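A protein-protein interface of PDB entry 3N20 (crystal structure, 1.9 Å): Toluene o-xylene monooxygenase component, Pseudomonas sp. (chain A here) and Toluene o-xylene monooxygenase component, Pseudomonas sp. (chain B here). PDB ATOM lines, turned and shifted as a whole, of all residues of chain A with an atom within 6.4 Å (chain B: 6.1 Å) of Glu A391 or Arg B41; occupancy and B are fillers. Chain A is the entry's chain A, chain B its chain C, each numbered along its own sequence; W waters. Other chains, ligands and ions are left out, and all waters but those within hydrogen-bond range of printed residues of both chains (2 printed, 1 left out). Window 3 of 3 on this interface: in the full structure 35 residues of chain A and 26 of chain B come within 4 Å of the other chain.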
ATOM      1  N   TYR A 337      -3.536 -24.343   1.140  1.00  0.00           N
ATOM      2  CA  TYR A 337      -4.038 -24.136  -0.213  1.00  0.00           C
ATOM      3  C   TYR A 337      -5.023 -22.970  -0.263  1.00  0.00           C
ATOM      4  O   TYR A 337      -5.030 -22.201  -1.225  1.00  0.00           O
ATOM      5  CB  TYR A 337      -4.710 -25.389  -0.773  1.00  0.00           C
ATOM      6  CG  TYR A 337      -4.782 -25.341  -2.283  1.00  0.00           C
ATOM      7  CD1 TYR A 337      -3.717 -25.795  -3.065  1.00  0.00           C
ATOM      8  CD2 TYR A 337      -5.878 -24.770  -2.932  1.00  0.00           C
ATOM      9  CE1 TYR A 337      -3.741 -25.676  -4.459  1.00  0.00           C
ATOM     10  CE2 TYR A 337      -5.907 -24.645  -4.325  1.00  0.00           C
ATOM     11  CZ  TYR A 337      -4.838 -25.100  -5.077  1.00  0.00           C
ATOM     12  OH  TYR A 337      -4.863 -24.979  -6.444  1.00  0.00           O
ATOM     13  N   TRP A 338      -5.851 -22.853   0.772  1.00  0.00           N
ATOM     14  CA  TRP A 338      -6.835 -21.776   0.876  1.00  0.00           C
ATOM     15  C   TRP A 338      -6.314 -20.657   1.786  1.00  0.00           C
ATOM     16  O   TRP A 338      -7.097 -19.960   2.436  1.00  0.00           O
ATOM     17  CB  TRP A 338      -8.150 -22.328   1.438  1.00  0.00           C
ATOM     18  CG  TRP A 338      -9.098 -22.812   0.380  1.00  0.00           C
ATOM     19  CD1 TRP A 338     -10.084 -22.088  -0.229  1.00  0.00           C
ATOM     20  CD2 TRP A 338      -9.111 -24.107  -0.235  1.00  0.00           C
ATOM     21  NE1 TRP A 338     -10.710 -22.852  -1.188  1.00  0.00           N
ATOM     22  CE2 TRP A 338     -10.136 -24.092  -1.213  1.00  0.00           C
ATOM     23  CE3 TRP A 338      -8.357 -25.278  -0.058  1.00  0.00           C
ATOM     24  CZ2 TRP A 338     -10.428 -25.208  -2.014  1.00  0.00           C
ATOM     25  CZ3 TRP A 338      -8.648 -26.390  -0.855  1.00  0.00           C
ATOM     26  CH2 TRP A 338      -9.679 -26.341  -1.825  1.00  0.00           C
ATOM     27  N   CYS A 372       0.302 -34.485  -3.445  1.00  0.00           N
ATOM     28  CA  CYS A 372      -0.407 -33.227  -3.653  1.00  0.00           C
ATOM     29  C   CYS A 372       0.650 -32.132  -3.601  1.00  0.00           C
ATOM     30  O   CYS A 372       0.695 -31.238  -4.449  1.00  0.00           O
ATOM     31  CB  CYS A 372      -1.434 -32.991  -2.541  1.00  0.00           C
ATOM     32  SG  CYS A 372      -2.830 -34.131  -2.541  1.00  0.00           S
ATOM     33  N   VAL A 375       2.834 -31.757  -6.786  1.00  0.00           N
ATOM     34  CA  VAL A 375       2.230 -30.953  -7.843  1.00  0.00           C
ATOM     35  C   VAL A 375       2.327 -29.467  -7.528  1.00  0.00           C
ATOM     36  O   VAL A 375       2.653 -28.660  -8.397  1.00  0.00           O
ATOM     37  CB  VAL A 375       0.749 -31.310  -8.042  1.00  0.00           C
ATOM     38  CG1 VAL A 375       0.164 -30.460  -9.153  1.00  0.00           C
ATOM     39  CG2 VAL A 375       0.608 -32.790  -8.372  1.00  0.00           C
ATOM     40  N   ILE A 376       2.035 -29.113  -6.281  1.00  0.00           N
ATOM     41  CA  ILE A 376       2.096 -27.724  -5.848  1.00  0.00           C
ATOM     42  C   ILE A 376       3.512 -27.175  -6.010  1.00  0.00           C
ATOM     43  O   ILE A 376       3.709 -26.062  -6.504  1.00  0.00           O
ATOM     44  CB  ILE A 376       1.658 -27.602  -4.370  1.00  0.00           C
ATOM     45  CG1 ILE A 376       0.149 -27.858  -4.264  1.00  0.00           C
ATOM     46  CG2 ILE A 376       2.049 -26.242  -3.814  1.00  0.00           C
ATOM     47  CD1 ILE A 376      -0.367 -28.018  -2.835  1.00  0.00           C
ATOM     48  N   ASN A 379       4.563 -26.573  -9.727  1.00  0.00           N
ATOM     49  CA  ASN A 379       3.950 -25.355 -10.250  1.00  0.00           C
ATOM     50  C   ASN A 379       4.677 -24.104  -9.772  1.00  0.00           C
ATOM     51  O   ASN A 379       4.825 -23.134 -10.523  1.00  0.00           O
ATOM     52  CB  ASN A 379       2.479 -25.292  -9.838  1.00  0.00           C
ATOM     53  CG  ASN A 379       1.600 -26.211 -10.669  1.00  0.00           C
ATOM     54  OD1 ASN A 379       0.595 -26.738 -10.187  1.00  0.00           O
ATOM     55  ND2 ASN A 379       1.967 -26.394 -11.932  1.00  0.00           N
ATOM     56  N   GLU A 386      -0.452 -19.360  -9.691  1.00  0.00           N
ATOM     57  CA  GLU A 386      -1.901 -19.272  -9.726  1.00  0.00           C
ATOM     58  C   GLU A 386      -2.585 -20.633  -9.566  1.00  0.00           C
ATOM     59  O   GLU A 386      -3.769 -20.698  -9.245  1.00  0.00           O
ATOM     60  CB  GLU A 386      -2.376 -18.590 -11.015  1.00  0.00           C
ATOM     61  CG  GLU A 386      -2.156 -19.378 -12.297  1.00  0.00           C
ATOM     62  CD  GLU A 386      -0.751 -19.230 -12.860  1.00  0.00           C
ATOM     63  OE1 GLU A 386       0.054 -18.452 -12.297  1.00  0.00           O
ATOM     64  OE2 GLU A 386      -0.455 -19.892 -13.879  1.00  0.00           O
ATOM     65  N   LEU A 387      -1.846 -21.717  -9.778  1.00  0.00           N
ATOM     66  CA  LEU A 387      -2.425 -23.051  -9.628  1.00  0.00           C
ATOM     67  C   LEU A 387      -2.283 -23.559  -8.194  1.00  0.00           C
ATOM     68  O   LEU A 387      -2.654 -24.702  -7.896  1.00  0.00           O
ATOM     69  CB  LEU A 387      -1.767 -24.046 -10.594  1.00  0.00           C
ATOM     70  CG  LEU A 387      -2.101 -23.899 -12.088  1.00  0.00           C
ATOM     71  CD1 LEU A 387      -1.247 -24.858 -12.901  1.00  0.00           C
ATOM     72  CD2 LEU A 387      -3.582 -24.170 -12.322  1.00  0.00           C
ATOM     73  N   THR A 388      -1.744 -22.711  -7.313  1.00  0.00           N
ATOM     74  CA  THR A 388      -1.561 -23.069  -5.904  1.00  0.00           C
ATOM     75  C   THR A 388      -2.566 -22.375  -4.977  1.00  0.00           C
ATOM     76  O   THR A 388      -2.473 -22.482  -3.754  1.00  0.00           O
ATOM     77  CB  THR A 388      -0.126 -22.764  -5.416  1.00  0.00           C
ATOM     78  OG1 THR A 388       0.090 -21.346  -5.380  1.00  0.00           O
ATOM     79  CG2 THR A 388       0.891 -23.407  -6.348  1.00  0.00           C
ATOM     80  N   VAL A 389      -3.509 -21.651  -5.574  1.00  0.00           N
ATOM     81  CA  VAL A 389      -4.576 -20.978  -4.837  1.00  0.00           C
ATOM     82  C   VAL A 389      -5.849 -21.473  -5.516  1.00  0.00           C
ATOM     83  O   VAL A 389      -5.844 -21.760  -6.714  1.00  0.00           O
ATOM     84  CB  VAL A 389      -4.465 -19.426  -4.902  1.00  0.00           C
ATOM     85  CG1 VAL A 389      -3.280 -18.967  -4.060  1.00  0.00           C
ATOM     86  CG2 VAL A 389      -4.308 -18.956  -6.341  1.00  0.00           C
ATOM     87  N   PRO A 390      -6.956 -21.574  -4.767  1.00  0.00           N
ATOM     88  CA  PRO A 390      -8.245 -22.057  -5.271  1.00  0.00           C
ATOM     89  C   PRO A 390      -9.148 -21.105  -6.031  1.00  0.00           C
ATOM     90  O   PRO A 390      -9.043 -19.885  -5.919  1.00  0.00           O
ATOM     91  CB  PRO A 390      -8.921 -22.552  -4.006  1.00  0.00           C
ATOM     92  CG  PRO A 390      -8.565 -21.441  -3.052  1.00  0.00           C
ATOM     93  CD  PRO A 390      -7.074 -21.187  -3.347  1.00  0.00           C
ATOM     94  N   GLU A 391     -10.061 -21.698  -6.794  1.00  0.00           N
ATOM     95  CA  GLU A 391     -11.032 -20.944  -7.565  1.00  0.00           C
ATOM     96  C   GLU A 391     -12.439 -21.422  -7.204  1.00  0.00           C
ATOM     97  O   GLU A 391     -13.411 -21.164  -7.912  1.00  0.00           O
ATOM     98  CB  GLU A 391     -10.746 -21.089  -9.063  1.00  0.00           C
ATOM     99  CG  GLU A 391      -9.474 -20.357  -9.472  1.00  0.00           C
ATOM    100  CD  GLU A 391      -9.215 -20.377 -10.967  1.00  0.00           C
ATOM    101  OE1 GLU A 391     -10.091 -19.924 -11.733  1.00  0.00           O
ATOM    102  OE2 GLU A 391      -8.128 -20.841 -11.375  1.00  0.00           O
ATOM    103  N   THR A 392     -12.532 -22.123  -6.078  1.00  0.00           N
ATOM    104  CA  THR A 392     -13.811 -22.609  -5.579  1.00  0.00           C
ATOM    105  C   THR A 392     -13.719 -22.859  -4.080  1.00  0.00           C
ATOM    106  O   THR A 392     -12.654 -22.713  -3.490  1.00  0.00           O
ATOM    107  CB  THR A 392     -14.243 -23.911  -6.276  1.00  0.00           C
ATOM    108  OG1 THR A 392     -15.585 -24.222  -5.882  1.00  0.00           O
ATOM    109  CG2 THR A 392     -13.318 -25.062  -5.899  1.00  0.00           C
ATOM    110  N   LEU A 393     -14.835 -23.228  -3.461  1.00  0.00           N
ATOM    111  CA  LEU A 393     -14.835 -23.505  -2.035  1.00  0.00           C
ATOM    112  C   LEU A 393     -14.772 -25.012  -1.831  1.00  0.00           C
ATOM    113  O   LEU A 393     -15.243 -25.783  -2.666  1.00  0.00           O
ATOM    114  CB  LEU A 393     -16.115 -23.013  -1.341  1.00  0.00           C
ATOM    115  CG  LEU A 393     -16.973 -21.795  -1.696  1.00  0.00           C
ATOM    116  CD1 LEU A 393     -17.516 -21.240  -0.378  1.00  0.00           C
ATOM    117  CD2 LEU A 393     -16.196 -20.717  -2.433  1.00  0.00           C
ATOM    118  N   LEU A 464     -15.748 -15.504  -5.440  1.00  0.00           N
ATOM    119  CA  LEU A 464     -14.693 -15.575  -4.440  1.00  0.00           C
ATOM    120  C   LEU A 464     -14.389 -14.234  -3.781  1.00  0.00           C
ATOM    121  O   LEU A 464     -14.150 -14.177  -2.574  1.00  0.00           O
ATOM    122  CB  LEU A 464     -13.421 -16.170  -5.056  1.00  0.00           C
ATOM    123  CG  LEU A 464     -13.561 -17.601  -5.590  1.00  0.00           C
ATOM    124  CD1 LEU A 464     -12.171 -18.187  -5.800  1.00  0.00           C
ATOM    125  CD2 LEU A 464     -14.339 -18.471  -4.611  1.00  0.00           C
ATOM    126  N   ALA B  35     -12.186 -31.700 -12.984  1.00  0.00           N
ATOM    127  CA  ALA B  35     -10.737 -31.818 -13.176  1.00  0.00           C
ATOM    128  C   ALA B  35     -10.044 -30.464 -13.060  1.00  0.00           C
ATOM    129  O   ALA B  35      -8.920 -30.366 -12.574  1.00  0.00           O
ATOM    130  CB  ALA B  35     -10.439 -32.430 -14.551  1.00  0.00           C
ATOM    131  N   TYR B  36     -10.720 -29.427 -13.531  1.00  0.00           N
ATOM    132  CA  TYR B  36     -10.199 -28.071 -13.482  1.00  0.00           C
ATOM    133  C   TYR B  36      -9.704 -27.707 -12.072  1.00  0.00           C
ATOM    134  O   TYR B  36      -8.700 -27.011 -11.915  1.00  0.00           O
ATOM    135  CB  TYR B  36     -11.301 -27.098 -13.910  1.00  0.00           C
ATOM    136  CG  TYR B  36     -10.873 -25.652 -13.940  1.00  0.00           C
ATOM    137  CD1 TYR B  36     -10.250 -25.109 -15.064  1.00  0.00           C
ATOM    138  CD2 TYR B  36     -11.060 -24.833 -12.831  1.00  0.00           C
ATOM    139  CE1 TYR B  36      -9.823 -23.778 -15.076  1.00  0.00           C
ATOM    140  CE2 TYR B  36     -10.636 -23.510 -12.832  1.00  0.00           C
ATOM    141  CZ  TYR B  36     -10.019 -22.990 -13.954  1.00  0.00           C
ATOM    142  OH  TYR B  36      -9.582 -21.689 -13.936  1.00  0.00           O
ATOM    143  N   HIS B  37     -10.403 -28.194 -11.049  1.00  0.00           N
ATOM    144  CA  HIS B  37     -10.044 -27.887  -9.666  1.00  0.00           C
ATOM    145  C   HIS B  37      -9.113 -28.880  -8.976  1.00  0.00           C
ATOM    146  O   HIS B  37      -8.791 -28.703  -7.802  1.00  0.00           O
ATOM    147  CB  HIS B  37     -11.316 -27.725  -8.836  1.00  0.00           C
ATOM    148  CG  HIS B  37     -12.216 -26.640  -9.335  1.00  0.00           C
ATOM    149  ND1 HIS B  37     -11.898 -25.303  -9.223  1.00  0.00           N
ATOM    150  CD2 HIS B  37     -13.400 -26.694  -9.990  1.00  0.00           C
ATOM    151  CE1 HIS B  37     -12.850 -24.581  -9.785  1.00  0.00           C
ATOM    152  NE2 HIS B  37     -13.772 -25.399 -10.260  1.00  0.00           N
ATOM    153  N   SER B  38      -8.671 -29.912  -9.693  1.00  0.00           N
ATOM    154  CA  SER B  38      -7.782 -30.902  -9.089  1.00  0.00           C
ATOM    155  C   SER B  38      -6.555 -31.251  -9.931  1.00  0.00           C
ATOM    156  O   SER B  38      -5.438 -31.286  -9.411  1.00  0.00           O
ATOM    157  CB  SER B  38      -8.562 -32.176  -8.765  1.00  0.00           C
ATOM    158  OG  SER B  38      -9.567 -31.917  -7.800  1.00  0.00           O
ATOM    159  N   ILE B  39      -6.761 -31.516 -11.220  1.00  0.00           N
ATOM    160  CA  ILE B  39      -5.657 -31.865 -12.115  1.00  0.00           C
ATOM    161  C   ILE B  39      -4.741 -30.656 -12.291  1.00  0.00           C
ATOM    162  O   ILE B  39      -5.208 -29.534 -12.513  1.00  0.00           O
ATOM    163  CB  ILE B  39      -6.179 -32.331 -13.507  1.00  0.00           C
ATOM    164  CG1 ILE B  39      -7.040 -33.591 -13.350  1.00  0.00           C
ATOM    165  CG2 ILE B  39      -5.005 -32.608 -14.451  1.00  0.00           C
ATOM    166  CD1 ILE B  39      -6.289 -34.806 -12.815  1.00  0.00           C
ATOM    167  N   ASN B  40      -3.439 -30.899 -12.177  1.00  0.00           N
ATOM    168  CA  ASN B  40      -2.420 -29.859 -12.298  1.00  0.00           C
ATOM    169  C   ASN B  40      -2.432 -28.844 -11.154  1.00  0.00           C
ATOM    170  O   ASN B  40      -1.798 -27.785 -11.225  1.00  0.00           O
ATOM    171  CB  ASN B  40      -2.523 -29.154 -13.656  1.00  0.00           C
ATOM    172  CG  ASN B  40      -2.096 -30.053 -14.791  1.00  0.00           C
ATOM    173  OD1 ASN B  40      -1.161 -30.851 -14.639  1.00  0.00           O
ATOM    174  ND2 ASN B  40      -2.759 -29.932 -15.936  1.00  0.00           N
ATOM    175  N   ARG B  41      -3.160 -29.178 -10.098  1.00  0.00           N
ATOM    176  CA  ARG B  41      -3.221 -28.332  -8.920  1.00  0.00           C
ATOM    177  C   ARG B  41      -2.727 -29.202  -7.768  1.00  0.00           C
ATOM    178  O   ARG B  41      -1.816 -28.823  -7.023  1.00  0.00           O
ATOM    179  CB  ARG B  41      -4.658 -27.874  -8.637  1.00  0.00           C
ATOM    180  CG  ARG B  41      -5.147 -26.734  -9.542  1.00  0.00           C
ATOM    181  CD  ARG B  41      -6.600 -26.384  -9.253  1.00  0.00           C
ATOM    182  NE  ARG B  41      -7.099 -25.300 -10.094  1.00  0.00           N
ATOM    183  CZ  ARG B  41      -6.836 -24.011  -9.898  1.00  0.00           C
ATOM    184  NH1 ARG B  41      -6.076 -23.627  -8.884  1.00  0.00           N
ATOM    185  NH2 ARG B  41      -7.338 -23.104 -10.723  1.00  0.00           N
ATOM    186  N   ARG B  42      -3.313 -30.394  -7.676  1.00  0.00           N
ATOM    187  CA  ARG B  42      -2.997 -31.357  -6.626  1.00  0.00           C
ATOM    188  C   ARG B  42      -2.905 -32.800  -7.122  1.00  0.00           C
ATOM    189  O   ARG B  42      -2.494 -33.690  -6.371  1.00  0.00           O
ATOM    190  CB  ARG B  42      -4.069 -31.306  -5.547  1.00  0.00           C
ATOM    191  CG  ARG B  42      -3.705 -30.474  -4.354  1.00  0.00           C
ATOM    192  CD  ARG B  42      -4.916 -30.292  -3.457  1.00  0.00           C
ATOM    193  NE  ARG B  42      -5.586 -29.049  -3.796  1.00  0.00           N
ATOM    194  CZ  ARG B  42      -6.812 -28.953  -4.287  1.00  0.00           C
ATOM    195  NH1 ARG B  42      -7.548 -30.036  -4.506  1.00  0.00           N
ATOM    196  NH2 ARG B  42      -7.295 -27.756  -4.565  1.00  0.00           N
ATOM    197  N   VAL B  43      -3.309 -33.037  -8.368  1.00  0.00           N
ATOM    198  CA  VAL B  43      -3.260 -34.374  -8.935  1.00  0.00           C
ATOM    199  C   VAL B  43      -2.648 -34.343 -10.328  1.00  0.00           C
ATOM    200  O   VAL B  43      -2.910 -33.430 -11.116  1.00  0.00           O
ATOM    201  CB  VAL B  43      -4.675 -34.988  -9.004  1.00  0.00           C
ATOM    202  CG1 VAL B  43      -4.601 -36.387  -9.562  1.00  0.00           C
ATOM    203  CG2 VAL B  43      -5.305 -34.997  -7.626  1.00  0.00           C
HETATM  204  O   HOH W   1      -9.668 -24.387  -7.522  1.00  0.00           O
HETATM  205  O   HOH W   2       1.513 -29.705 -12.717  1.00  0.00           O
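NH1 of Arg B41 is in hydrogen-bond range of OH of Tyr A337 (3.0 Å).
The side-chain amide oxygen (OD1) of Asn A379 sits close to the backbone carbonyl oxygen (O) of Asn B40 (2.8 Å).
The guanidinium group (NH1) of Arg B41 sits at hydrogen-bond distance from the backbone carbonyl oxygen (O) of Val A389 (2.9 Å).
The side-chain hydroxyl (OH) of Tyr B36 sits at hydrogen-bond distance from the side-chain carboxylate (OE1) of Glu A391 (2.9 Å).
OE2 of Glu A391 lies within salt-bridge range of NH2 of Arg B41 (2.5 Å).
The side-chain hydroxyl (OH) of Tyr A337 is in hydrogen-bond range of the backbone carbonyl oxygen (O) of Leu A387 (2.7 Å).
OH of Tyr A337 lies within hydrogen-bond range of O of Val A389, 3.4 Å away.
O of Thr A392 sits at hydrogen-bond distance from NE1 of Trp A338 (3.0 Å).
The backbone carbonyl oxygen of Val A375 sits close to the side-chain amide oxygen of Asn A379 (3.3 Å).
The backbone carbonyl oxygen of Tyr B36 sits at hydrogen-bond distance from the guanidinium group of Arg B41, at 3.0 Å.
The backbone carbonyl oxygen of Ser B38 lies within hydrogen-bond range of the backbone NH of Val B43 (2.9 Å).
Among the printed residues, merely in contact across the chains: Tyr A337 with Arg B42, Trp A338 with Arg B42, Cys A372 with Arg B42, Val A375 with Asn B40, Val A375 with Arg B41, Val A375 with Arg B42, Val A375 with Val B43, Ile A376 with Arg B41, Glu A386 with Arg B41, Leu A387 with Asn B40, Leu A387 with Arg B41, Glu A391 with His B37 and Thr A392 with His B37.
Glu A391 touches just these residues of chain B: Tyr B36 (2.9 Å), His B37 (3.9 Å) and Arg B41 (2.5 Å).
Of chain A, only Tyr A337, Val A375, Ile A376, Glu A386, Leu A387, Val A389 and Glu A391 come within 4 Å of Arg B41.
Printed residues of chain B within 4 Å of Asn A379: Asn B40.
Of the printed residues of chain B, Thr A392 touches His B37.
Thr A388 touches none of the printed residues of chain B.
Pro A390 touches none of the printed residues of chain B.
The nearest printed residue of chain B that does not touch Glu A391 is Arg B42 (7.0 Å).
Of the 9 printed residues of chain B, 6 touch a printed residue of chain A.
Hydrophobic or aromatic side chains of chain A that line the printed part of chain B: Tyr A337, Trp A338, Val A375, Ile A376 and Leu A387.
Water W1 bridges N of Glu A391 and ND1 of His B37.
Water W2 bridges ND2 of Asn A379 (3.4 Å) and OD1 of Asn B40 (3.5 Å).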
